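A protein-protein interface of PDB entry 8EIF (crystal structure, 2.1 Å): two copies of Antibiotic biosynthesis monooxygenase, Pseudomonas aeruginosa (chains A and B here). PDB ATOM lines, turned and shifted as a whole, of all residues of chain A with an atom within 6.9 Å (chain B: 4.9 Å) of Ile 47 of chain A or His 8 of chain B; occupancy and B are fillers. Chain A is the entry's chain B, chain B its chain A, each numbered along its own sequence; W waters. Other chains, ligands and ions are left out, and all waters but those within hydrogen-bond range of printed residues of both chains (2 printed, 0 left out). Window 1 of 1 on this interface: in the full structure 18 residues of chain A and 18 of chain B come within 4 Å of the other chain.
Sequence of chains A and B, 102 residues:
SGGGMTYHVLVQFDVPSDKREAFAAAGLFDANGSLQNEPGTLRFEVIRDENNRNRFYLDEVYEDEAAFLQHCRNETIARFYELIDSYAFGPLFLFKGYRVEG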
ATOM      1  N   LEU A  10      -5.858   2.698  16.703  1.00  0.00           N
ATOM      2  CA  LEU A  10      -5.078   1.468  16.623  1.00  0.00           C
ATOM      3  C   LEU A  10      -3.793   1.744  15.854  1.00  0.00           C
ATOM      4  O   LEU A  10      -3.840   2.200  14.707  1.00  0.00           O
ATOM      5  CB  LEU A  10      -5.888   0.359  15.951  1.00  0.00           C
ATOM      6  CG  LEU A  10      -6.520  -0.681  16.877  1.00  0.00           C
ATOM      7  CD1 LEU A  10      -5.459  -1.367  17.717  1.00  0.00           C
ATOM      8  CD2 LEU A  10      -7.554  -0.018  17.777  1.00  0.00           C
ATOM      9  N   VAL A  11      -2.649   1.457  16.483  1.00  0.00           N
ATOM     10  CA  VAL A  11      -1.337   1.823  15.962  1.00  0.00           C
ATOM     11  C   VAL A  11      -0.460   0.580  15.853  1.00  0.00           C
ATOM     12  O   VAL A  11      -0.556  -0.342  16.668  1.00  0.00           O
ATOM     13  CB  VAL A  11      -0.659   2.886  16.855  1.00  0.00           C
ATOM     14  CG1 VAL A  11       0.491   3.531  16.125  1.00  0.00           C
ATOM     15  CG2 VAL A  11      -1.670   3.942  17.303  1.00  0.00           C
ATOM     16  N   PHE A  23      11.324  -2.082  23.200  1.00  0.00           N
ATOM     17  CA  PHE A  23      10.078  -1.458  22.766  1.00  0.00           C
ATOM     18  C   PHE A  23       8.937  -1.768  23.725  1.00  0.00           C
ATOM     19  O   PHE A  23       8.066  -0.920  23.954  1.00  0.00           O
ATOM     20  CB  PHE A  23       9.705  -1.900  21.351  1.00  0.00           C
ATOM     21  CG  PHE A  23       8.441  -1.264  20.854  1.00  0.00           C
ATOM     22  CD1 PHE A  23       8.476  -0.022  20.243  1.00  0.00           C
ATOM     23  CD2 PHE A  23       7.213  -1.886  21.031  1.00  0.00           C
ATOM     24  CE1 PHE A  23       7.314   0.580  19.800  1.00  0.00           C
ATOM     25  CE2 PHE A  23       6.051  -1.284  20.594  1.00  0.00           C
ATOM     26  CZ  PHE A  23       6.102  -0.051  19.973  1.00  0.00           C
ATOM     27  N   GLU A  45      -3.410  -0.059  25.528  1.00  0.00           N
ATOM     28  CA  GLU A  45      -2.902  -1.420  25.606  1.00  0.00           C
ATOM     29  C   GLU A  45      -1.764  -1.649  24.619  1.00  0.00           C
ATOM     30  O   GLU A  45      -1.827  -1.217  23.465  1.00  0.00           O
ATOM     31  CB  GLU A  45      -4.019  -2.447  25.369  1.00  0.00           C
ATOM     32  CG  GLU A  45      -4.992  -2.553  26.535  1.00  0.00           C
ATOM     33  CD  GLU A  45      -6.157  -3.482  26.258  1.00  0.00           C
ATOM     34  OE1 GLU A  45      -6.480  -3.702  25.073  1.00  0.00           O
ATOM     35  OE2 GLU A  45      -6.751  -3.992  27.233  1.00  0.00           O
ATOM     36  N   VAL A  46      -0.726  -2.333  25.097  1.00  0.00           N
ATOM     37  CA  VAL A  46       0.397  -2.778  24.282  1.00  0.00           C
ATOM     38  C   VAL A  46       0.196  -4.259  23.992  1.00  0.00           C
ATOM     39  O   VAL A  46       0.082  -5.072  24.917  1.00  0.00           O
ATOM     40  CB  VAL A  46       1.739  -2.532  24.989  1.00  0.00           C
ATOM     41  CG1 VAL A  46       2.901  -2.944  24.093  1.00  0.00           C
ATOM     42  CG2 VAL A  46       1.862  -1.067  25.397  1.00  0.00           C
ATOM     43  N   ILE A  47       0.145  -4.609  22.709  1.00  0.00           N
ATOM     44  CA  ILE A  47      -0.175  -5.961  22.266  1.00  0.00           C
ATOM     45  C   ILE A  47       0.898  -6.412  21.285  1.00  0.00           C
ATOM     46  O   ILE A  47       1.269  -5.657  20.378  1.00  0.00           O
ATOM     47  CB  ILE A  47      -1.567  -6.026  21.608  1.00  0.00           C
ATOM     48  CG1 ILE A  47      -2.642  -5.516  22.573  1.00  0.00           C
ATOM     49  CG2 ILE A  47      -1.885  -7.448  21.149  1.00  0.00           C
ATOM     50  CD1 ILE A  47      -3.927  -5.104  21.886  1.00  0.00           C
ATOM     51  N   ARG A  48       1.395  -7.634  21.462  1.00  0.00           N
ATOM     52  CA  ARG A  48       2.328  -8.230  20.514  1.00  0.00           C
ATOM     53  C   ARG A  48       1.609  -9.226  19.618  1.00  0.00           C
ATOM     54  O   ARG A  48       0.748  -9.981  20.077  1.00  0.00           O
ATOM     55  CB  ARG A  48       3.491  -8.933  21.216  1.00  0.00           C
ATOM     56  CG  ARG A  48       4.519  -9.449  20.210  1.00  0.00           C
ATOM     57  CD  ARG A  48       5.944  -9.347  20.694  1.00  0.00           C
ATOM     58  NE  ARG A  48       6.250 -10.233  21.809  1.00  0.00           N
ATOM     59  CZ  ARG A  48       7.319 -11.014  21.855  1.00  0.00           C
ATOM     60  NH1 ARG A  48       8.206 -11.028  20.872  1.00  0.00           N
ATOM     61  NH2 ARG A  48       7.509 -11.794  22.915  1.00  0.00           N
ATOM     62  N   ASP A  49       1.980  -9.224  18.340  1.00  0.00           N
ATOM     63  CA  ASP A  49       1.415 -10.165  17.380  1.00  0.00           C
ATOM     64  C   ASP A  49       1.719 -11.600  17.799  1.00  0.00           C
ATOM     65  O   ASP A  49       2.800 -11.900  18.309  1.00  0.00           O
ATOM     66  CB  ASP A  49       1.982  -9.884  15.987  1.00  0.00           C
ATOM     67  CG  ASP A  49       1.216 -10.589  14.889  1.00  0.00           C
ATOM     68  OD1 ASP A  49       0.230 -10.008  14.389  1.00  0.00           O
ATOM     69  OD2 ASP A  49       1.602 -11.720  14.522  1.00  0.00           O
ATOM     70  N   GLU A  50       0.752 -12.496  17.570  1.00  0.00           N
ATOM     71  CA  GLU A  50       0.889 -13.874  18.040  1.00  0.00           C
ATOM     72  C   GLU A  50       1.967 -14.640  17.282  1.00  0.00           C
ATOM     73  O   GLU A  50       2.538 -15.594  17.822  1.00  0.00           O
ATOM     74  CB  GLU A  50      -0.450 -14.604  17.927  1.00  0.00           C
ATOM     75  CG  GLU A  50      -0.941 -14.792  16.498  1.00  0.00           C
ATOM     76  CD  GLU A  50      -2.265 -15.533  16.421  1.00  0.00           C
ATOM     77  OE1 GLU A  50      -2.775 -15.965  17.477  1.00  0.00           O
ATOM     78  OE2 GLU A  50      -2.795 -15.687  15.302  1.00  0.00           O
ATOM     79  N   ARG A  55       6.520  -7.423  15.646  1.00  0.00           N
ATOM     80  CA  ARG A  55       5.404  -6.519  15.399  1.00  0.00           C
ATOM     81  C   ARG A  55       4.602  -6.305  16.676  1.00  0.00           C
ATOM     82  O   ARG A  55       4.210  -7.272  17.340  1.00  0.00           O
ATOM     83  CB  ARG A  55       4.503  -7.063  14.285  1.00  0.00           C
ATOM     84  CG  ARG A  55       3.311  -6.170  13.963  1.00  0.00           C
ATOM     85  CD  ARG A  55       2.857  -6.349  12.523  1.00  0.00           C
ATOM     86  NE  ARG A  55       3.777  -5.727  11.577  1.00  0.00           N
ATOM     87  CZ  ARG A  55       3.581  -5.666  10.267  1.00  0.00           C
ATOM     88  NH1 ARG A  55       2.506  -6.189   9.705  1.00  0.00           N
ATOM     89  NH2 ARG A  55       4.488  -5.065   9.502  1.00  0.00           N
ATOM     90  N   PHE A  56       4.358  -5.037  17.010  1.00  0.00           N
ATOM     91  CA  PHE A  56       3.590  -4.648  18.184  1.00  0.00           C
ATOM     92  C   PHE A  56       2.451  -3.728  17.771  1.00  0.00           C
ATOM     93  O   PHE A  56       2.541  -3.017  16.767  1.00  0.00           O
ATOM     94  CB  PHE A  56       4.448  -3.912  19.219  1.00  0.00           C
ATOM     95  CG  PHE A  56       5.463  -4.774  19.912  1.00  0.00           C
ATOM     96  CD1 PHE A  56       6.602  -5.200  19.249  1.00  0.00           C
ATOM     97  CD2 PHE A  56       5.293  -5.130  21.240  1.00  0.00           C
ATOM     98  CE1 PHE A  56       7.543  -5.983  19.893  1.00  0.00           C
ATOM     99  CE2 PHE A  56       6.231  -5.910  21.890  1.00  0.00           C
ATOM    100  CZ  PHE A  56       7.359  -6.333  21.218  1.00  0.00           C
ATOM    101  N   TYR A  57       1.388  -3.722  18.574  1.00  0.00           N
ATOM    102  CA  TYR A  57       0.260  -2.828  18.359  1.00  0.00           C
ATOM    103  C   TYR A  57      -0.060  -2.067  19.637  1.00  0.00           C
ATOM    104  O   TYR A  57       0.143  -2.568  20.748  1.00  0.00           O
ATOM    105  CB  TYR A  57      -0.994  -3.586  17.898  1.00  0.00           C
ATOM    106  CG  TYR A  57      -0.724  -4.612  16.829  1.00  0.00           C
ATOM    107  CD1 TYR A  57      -0.653  -4.247  15.491  1.00  0.00           C
ATOM    108  CD2 TYR A  57      -0.530  -5.947  17.158  1.00  0.00           C
ATOM    109  CE1 TYR A  57      -0.400  -5.187  14.510  1.00  0.00           C
ATOM    110  CE2 TYR A  57      -0.278  -6.892  16.185  1.00  0.00           C
ATOM    111  CZ  TYR A  57      -0.215  -6.507  14.865  1.00  0.00           C
ATOM    112  OH  TYR A  57       0.037  -7.453  13.900  1.00  0.00           O
ATOM    113  N   LEU A  58      -0.570  -0.850  19.466  1.00  0.00           N
ATOM    114  CA  LEU A  58      -1.080  -0.037  20.563  1.00  0.00           C
ATOM    115  C   LEU A  58      -2.576   0.161  20.363  1.00  0.00           C
ATOM    116  O   LEU A  58      -3.004   0.665  19.319  1.00  0.00           O
ATOM    117  CB  LEU A  58      -0.366   1.315  20.639  1.00  0.00           C
ATOM    118  CG  LEU A  58       1.163   1.341  20.680  1.00  0.00           C
ATOM    119  CD1 LEU A  58       1.667   2.780  20.806  1.00  0.00           C
ATOM    120  CD2 LEU A  58       1.687   0.487  21.821  1.00  0.00           C
ATOM    121  N   ASP A  59      -3.366  -0.236  21.357  1.00  0.00           N
ATOM    122  CA  ASP A  59      -4.817  -0.093  21.329  1.00  0.00           C
ATOM    123  C   ASP A  59      -5.187   1.003  22.323  1.00  0.00           C
ATOM    124  O   ASP A  59      -5.145   0.785  23.539  1.00  0.00           O
ATOM    125  CB  ASP A  59      -5.501  -1.419  21.665  1.00  0.00           C
ATOM    126  CG  ASP A  59      -6.974  -1.433  21.289  1.00  0.00           C
ATOM    127  OD1 ASP A  59      -7.568  -0.344  21.141  1.00  0.00           O
ATOM    128  OD2 ASP A  59      -7.538  -2.538  21.138  1.00  0.00           O
ATOM    129  N   THR B   6      -3.971 -11.331  28.120  1.00  0.00           N
ATOM    130  CA  THR B   6      -5.199 -11.639  27.405  1.00  0.00           C
ATOM    131  C   THR B   6      -4.928 -11.764  25.905  1.00  0.00           C
ATOM    132  O   THR B   6      -3.865 -11.394  25.398  1.00  0.00           O
ATOM    133  CB  THR B   6      -6.259 -10.572  27.676  1.00  0.00           C
ATOM    134  OG1 THR B   6      -5.674  -9.269  27.566  1.00  0.00           O
ATOM    135  CG2 THR B   6      -6.840 -10.749  29.072  1.00  0.00           C
ATOM    136  N   TYR B   7      -5.918 -12.301  25.195  1.00  0.00           N
ATOM    137  CA  TYR B   7      -5.824 -12.605  23.771  1.00  0.00           C
ATOM    138  C   TYR B   7      -6.753 -11.664  23.012  1.00  0.00           C
ATOM    139  O   TYR B   7      -7.955 -11.615  23.294  1.00  0.00           O
ATOM    140  CB  TYR B   7      -6.190 -14.069  23.520  1.00  0.00           C
ATOM    141  CG  TYR B   7      -5.957 -14.571  22.113  1.00  0.00           C
ATOM    142  CD1 TYR B   7      -4.671 -14.751  21.620  1.00  0.00           C
ATOM    143  CD2 TYR B   7      -7.028 -14.895  21.287  1.00  0.00           C
ATOM    144  CE1 TYR B   7      -4.458 -15.225  20.334  1.00  0.00           C
ATOM    145  CE2 TYR B   7      -6.826 -15.368  20.003  1.00  0.00           C
ATOM    146  CZ  TYR B   7      -5.542 -15.531  19.532  1.00  0.00           C
ATOM    147  OH  TYR B   7      -5.342 -16.003  18.255  1.00  0.00           O
ATOM    148  N   HIS B   8      -6.199 -10.923  22.052  1.00  0.00           N
ATOM    149  CA  HIS B   8      -6.903  -9.835  21.385  1.00  0.00           C
ATOM    150  C   HIS B   8      -7.047 -10.124  19.895  1.00  0.00           C
ATOM    151  O   HIS B   8      -6.097 -10.570  19.247  1.00  0.00           O
ATOM    152  CB  HIS B   8      -6.164  -8.505  21.596  1.00  0.00           C
ATOM    153  CG  HIS B   8      -6.003  -8.129  23.037  1.00  0.00           C
ATOM    154  ND1 HIS B   8      -6.612  -7.025  23.592  1.00  0.00           N
ATOM    155  CD2 HIS B   8      -5.312  -8.721  24.041  1.00  0.00           C
ATOM    156  CE1 HIS B   8      -6.299  -6.949  24.873  1.00  0.00           C
ATOM    157  NE2 HIS B   8      -5.513  -7.967  25.172  1.00  0.00           N
ATOM    158  N   VAL B   9      -8.235  -9.854  19.355  1.00  0.00           N
ATOM    159  CA  VAL B   9      -8.574 -10.164  17.966  1.00  0.00           C
ATOM    160  C   VAL B   9      -9.240  -8.941  17.345  1.00  0.00           C
ATOM    161  O   VAL B   9     -10.278  -8.480  17.834  1.00  0.00           O
ATOM    162  CB  VAL B   9      -9.496 -11.392  17.863  1.00  0.00           C
ATOM    163  CG1 VAL B   9      -9.900 -11.644  16.415  1.00  0.00           C
ATOM    164  CG2 VAL B   9      -8.822 -12.623  18.459  1.00  0.00           C
ATOM    165  N   LEU B  10      -8.655  -8.427  16.263  1.00  0.00           N
ATOM    166  CA  LEU B  10      -9.132  -7.224  15.587  1.00  0.00           C
ATOM    167  C   LEU B  10      -9.618  -7.604  14.193  1.00  0.00           C
ATOM    168  O   LEU B  10      -8.855  -8.166  13.401  1.00  0.00           O
ATOM    169  CB  LEU B  10      -8.021  -6.175  15.506  1.00  0.00           C
ATOM    170  CG  LEU B  10      -8.006  -5.066  16.561  1.00  0.00           C
ATOM    171  CD1 LEU B  10      -9.254  -4.198  16.462  1.00  0.00           C
ATOM    172  CD2 LEU B  10      -7.866  -5.653  17.959  1.00  0.00           C
ATOM    173  N   ARG B  43     -14.252  -8.809  26.350  1.00  0.00           N
ATOM    174  CA  ARG B  43     -14.519  -7.494  25.784  1.00  0.00           C
ATOM    175  C   ARG B  43     -14.857  -7.666  24.309  1.00  0.00           C
ATOM    176  O   ARG B  43     -14.286  -8.526  23.635  1.00  0.00           O
ATOM    177  CB  ARG B  43     -13.313  -6.561  25.964  1.00  0.00           C
ATOM    178  CG  ARG B  43     -13.658  -5.084  26.064  1.00  0.00           C
ATOM    179  CD  ARG B  43     -12.448  -4.272  26.513  1.00  0.00           C
ATOM    180  NE  ARG B  43     -11.464  -4.127  25.447  1.00  0.00           N
ATOM    181  CZ  ARG B  43     -10.152  -4.074  25.636  1.00  0.00           C
ATOM    182  NH1 ARG B  43      -9.624  -4.145  26.847  1.00  0.00           N
ATOM    183  NH2 ARG B  43      -9.350  -3.952  24.582  1.00  0.00           N
ATOM    184  N   GLU B  60     -12.038  -7.466  19.885  1.00  0.00           N
ATOM    185  CA  GLU B  60     -12.425  -8.585  20.734  1.00  0.00           C
ATOM    186  C   GLU B  60     -11.272  -8.993  21.644  1.00  0.00           C
ATOM    187  O   GLU B  60     -10.123  -9.085  21.203  1.00  0.00           O
ATOM    188  CB  GLU B  60     -12.857  -9.780  19.881  1.00  0.00           C
ATOM    189  CG  GLU B  60     -13.644  -9.405  18.633  1.00  0.00           C
ATOM    190  CD  GLU B  60     -13.999 -10.611  17.783  1.00  0.00           C
ATOM    191  OE1 GLU B  60     -13.660 -11.744  18.188  1.00  0.00           O
ATOM    192  OE2 GLU B  60     -14.608 -10.424  16.709  1.00  0.00           O
ATOM    193  N   VAL B  61     -11.587  -9.246  22.914  1.00  0.00           N
ATOM    194  CA  VAL B  61     -10.609  -9.677  23.906  1.00  0.00           C
ATOM    195  C   VAL B  61     -11.118 -10.950  24.567  1.00  0.00           C
ATOM    196  O   VAL B  61     -12.305 -11.056  24.898  1.00  0.00           O
ATOM    197  CB  VAL B  61     -10.341  -8.585  24.963  1.00  0.00           C
ATOM    198  CG1 VAL B  61      -9.234  -9.023  25.913  1.00  0.00           C
ATOM    199  CG2 VAL B  61      -9.977  -7.273  24.290  1.00  0.00           C
ATOM    200  N   PHE B  95      -5.315  -8.574  13.026  1.00  0.00           N
ATOM    201  CA  PHE B  95      -4.291  -9.289  13.771  1.00  0.00           C
ATOM    202  C   PHE B  95      -4.930 -10.033  14.932  1.00  0.00           C
ATOM    203  O   PHE B  95      -6.086  -9.798  15.291  1.00  0.00           O
ATOM    204  CB  PHE B  95      -3.182  -8.344  14.275  1.00  0.00           C
ATOM    205  CG  PHE B  95      -3.635  -7.350  15.320  1.00  0.00           C
ATOM    206  CD1 PHE B  95      -3.763  -7.716  16.654  1.00  0.00           C
ATOM    207  CD2 PHE B  95      -3.909  -6.039  14.964  1.00  0.00           C
ATOM    208  CE1 PHE B  95      -4.170  -6.797  17.606  1.00  0.00           C
ATOM    209  CE2 PHE B  95      -4.316  -5.116  15.911  1.00  0.00           C
ATOM    210  CZ  PHE B  95      -4.444  -5.495  17.235  1.00  0.00           C
ATOM    211  N   LYS B  96      -4.151 -10.948  15.499  1.00  0.00           N
ATOM    212  CA  LYS B  96      -4.431 -11.566  16.784  1.00  0.00           C
ATOM    213  C   LYS B  96      -3.142 -11.548  17.588  1.00  0.00           C
ATOM    214  O   LYS B  96      -2.056 -11.721  17.027  1.00  0.00           O
ATOM    215  CB  LYS B  96      -4.959 -13.001  16.630  1.00  0.00           C
ATOM    216  CG  LYS B  96      -6.111 -13.126  15.638  1.00  0.00           C
ATOM    217  CD  LYS B  96      -6.837 -14.449  15.775  1.00  0.00           C
ATOM    218  CE  LYS B  96      -6.351 -15.445  14.744  1.00  0.00           C
ATOM    219  NZ  LYS B  96      -6.911 -15.166  13.394  1.00  0.00           N
ATOM    220  N   GLY B  97      -3.254 -11.318  18.892  1.00  0.00           N
ATOM    221  CA  GLY B  97      -2.042 -11.186  19.680  1.00  0.00           C
ATOM    222  C   GLY B  97      -2.311 -11.260  21.167  1.00  0.00           C
ATOM    223  O   GLY B  97      -3.442 -11.472  21.612  1.00  0.00           O
ATOM    224  N   TYR B  98      -1.237 -11.071  21.930  1.00  0.00           N
ATOM    225  CA  TYR B  98      -1.241 -11.220  23.377  1.00  0.00           C
ATOM    226  C   TYR B  98      -0.881  -9.893  24.028  1.00  0.00           C
ATOM    227  O   TYR B  98       0.036  -9.198  23.579  1.00  0.00           O
ATOM    228  CB  TYR B  98      -0.251 -12.307  23.816  1.00  0.00           C
ATOM    229  CG  TYR B  98      -0.665 -13.703  23.409  1.00  0.00           C
ATOM    230  CD1 TYR B  98      -1.557 -14.436  24.181  1.00  0.00           C
ATOM    231  CD2 TYR B  98      -0.175 -14.281  22.244  1.00  0.00           C
ATOM    232  CE1 TYR B  98      -1.943 -15.713  23.811  1.00  0.00           C
ATOM    233  CE2 TYR B  98      -0.556 -15.559  21.864  1.00  0.00           C
ATOM    234  CZ  TYR B  98      -1.440 -16.269  22.653  1.00  0.00           C
ATOM    235  OH  TYR B  98      -1.827 -17.538  22.284  1.00  0.00           O
ATOM    236  N   ARG B  99      -1.604  -9.546  25.091  1.00  0.00           N
ATOM    237  CA  ARG B  99      -1.373  -8.279  25.770  1.00  0.00           C
ATOM    238  C   ARG B  99      -0.062  -8.314  26.546  1.00  0.00           C
ATOM    239  O   ARG B  99       0.229  -9.281  27.256  1.00  0.00           O
ATOM    240  CB  ARG B  99      -2.531  -7.958  26.712  1.00  0.00           C
ATOM    241  CG  ARG B  99      -2.364  -6.646  27.474  1.00  0.00           C
ATOM    242  CD  ARG B  99      -3.642  -6.255  28.204  1.00  0.00           C
ATOM    243  NE  ARG B  99      -3.426  -5.184  29.171  1.00  0.00           N
ATOM    244  CZ  ARG B  99      -4.366  -4.708  29.977  1.00  0.00           C
ATOM    245  NH1 ARG B  99      -5.604  -5.167  29.938  1.00  0.00           N
ATOM    246  NH2 ARG B  99      -4.054  -3.750  30.846  1.00  0.00           N
ATOM    247  N   VAL B 100       0.724  -7.251  26.412  1.00  0.00           N
ATOM    248  CA  VAL B 100       1.988  -7.117  27.125  1.00  0.00           C
ATOM    249  C   VAL B 100       1.710  -6.476  28.478  1.00  0.00           C
ATOM    250  O   VAL B 100       1.165  -5.371  28.549  1.00  0.00           O
ATOM    251  CB  VAL B 100       2.993  -6.283  26.316  1.00  0.00           C
ATOM    252  CG1 VAL B 100       4.231  -5.988  27.152  1.00  0.00           C
ATOM    253  CG2 VAL B 100       3.362  -7.000  25.025  1.00  0.00           C
HETATM  254  O   HOH W   1      -7.008  -2.495  29.666  1.00  0.00           O
HETATM  255  O   HOH W   2      -7.645  -5.248  21.870  1.00  0.00           O
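N of Tyr 98 of chain B lies within hydrogen-bond range of O of Arg 48 of chain A, at 2.9 Å.
The side-chain carboxylate (OE1) of Glu 50 of chain A lies within hydrogen-bond range of the side-chain hydroxyl (OH) of Tyr 7 of chain B, 2.7 Å away.
The backbone NH (N) of Glu 50 of chain A sits at hydrogen-bond distance from the backbone carbonyl oxygen (O) of Lys 96 of chain B (3.0 Å).
The guanidinium group of Arg 43 of chain B lies within salt-bridge range of the side-chain carboxylate of Glu 45 of chain A (2.9 Å).
N of Val 100 of chain B is in hydrogen-bond range of O of Val 46 of chain A.
The side-chain carboxylate of Glu 45 of chain A is in salt-bridge range of the guanidinium group of Arg 99 of chain B, at 3.2 Å.
The backbone NH (N) of Tyr 57 of chain A lies within hydrogen-bond range of the backbone carbonyl oxygen (O) of Ile 47 of chain A (2.6 Å).
The side-chain hydroxyl (OH) of Tyr 57 of chain A lies within hydrogen-bond range of the side-chain carboxylate (OD1) of Asp 49 of chain A.
The backbone NH of Leu 10 of chain B is in hydrogen-bond range of the backbone carbonyl oxygen of Phe 95 of chain B (3.1 Å).
A ring nitrogen (NE2) of His 8 of chain B sits at hydrogen-bond distance from the side-chain hydroxyl of Thr 6 of chain B, 2.7 Å away.
The backbone carbonyl oxygen (O) of Asp 59 of chain A sits at hydrogen-bond distance from the backbone NH (N) of Glu 45 of chain A (2.8 Å).
The backbone NH of Asp 49 of chain A is in hydrogen-bond range of the backbone carbonyl oxygen of Arg 55 of chain A.
Glu 45 of chain A touches His 8 of chain B (OE1 to CE1, 3.3 Å).
Val 46 of chain A touches Arg 99 of chain B.
ND1 of His 8 of chain B touches CD1 of Ile 47 of chain A, 3.7 Å away.
Ile 47 of chain A touches Gly 97 of chain B (CG2 to C, 3.8 Å).
Tyr 98 of chain B touches Ile 47 of chain A (O to CA, 3.5 Å).
O of Arg 48 of chain A touches CA of Gly 97 of chain B (3.1 Å).
Phe 95 of chain B touches Asp 49 of chain A (CB to OD1, 3.8 Å).
O of Lys 96 of chain B touches CA of Asp 49 of chain A, 3.8 Å away.
Gly 97 of chain B touches Glu 50 of chain A.
OH of Tyr 57 of chain A touches CB of Phe 95 of chain B (3.4 Å).
Ile 47 of chain A touches just these residues of chain B: His 8, Gly 97 and Tyr 98.
His 8 of chain B touches two residues of chain A.
Of the printed residues of chain B, Tyr 57 of chain A touches Phe 95 (3.4 Å).
Printed residues of chain B within 4 Å of Arg 48 of chain A: Gly 97 (3.1 Å) and Tyr 98 (2.9 Å).
Asp 59 of chain A touches none of the printed residues of chain B.
Leu 10 of chain B touches none of the printed residues of chain A.
The nearest residue of chain B that does not touch Ile 47 of chain A is Phe 95 of chain B (4.3 Å).
The nearest printed residue of chain A that does not touch Arg 99 of chain B is Ile 47 of chain A (4.4 Å).
Of the 14 printed residues of chain B, 9 touch a printed residue of chain A.
Hydrophobic or aromatic side chains of chain B within 4 Å of the printed part of chain A: Tyr 7, His 8, Phe 95 and Val 100.
Of the 14 printed residues of chain A, 7 touch a printed residue of chain B.
Printed residues of chain A that touch a printed residue of chain B: Glu 45, Val 46, Ile 47, Arg 48, Asp 49, Glu 50 and Tyr 57.
Hydrophobic or aromatic side chains of chain A within 4 Å of the printed part of chain B: Ile 47 and Tyr 57.
Among the printed residues, Asp or Glu carboxylates within 4 Å of a Lys or Arg side-chain nitrogen of the other chain: Glu 45 of chain A with Arg 43 of chain B and Glu 45 of chain A with Arg 99 of chain B.
Position printed for both chains: 10.
Of the 16 pairs that touch across the chains among the printed residues, none has its exchanged pair printed and touching as well.
Water W2 lies within hydrogen-bond range of ND1 of His 8 of chain B (2.7 Å), OD2 of Asp 59 of chain A (2.8 Å) and NH2 of Arg 43 of chain B (3.5 Å).
Water W1 lies within hydrogen-bond range of the side-chain carboxylate (OE2) of Glu 45 of chain A (2.9 Å) and the guanidinium group (NH1) of Arg 99 of chain B (3.0 Å).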
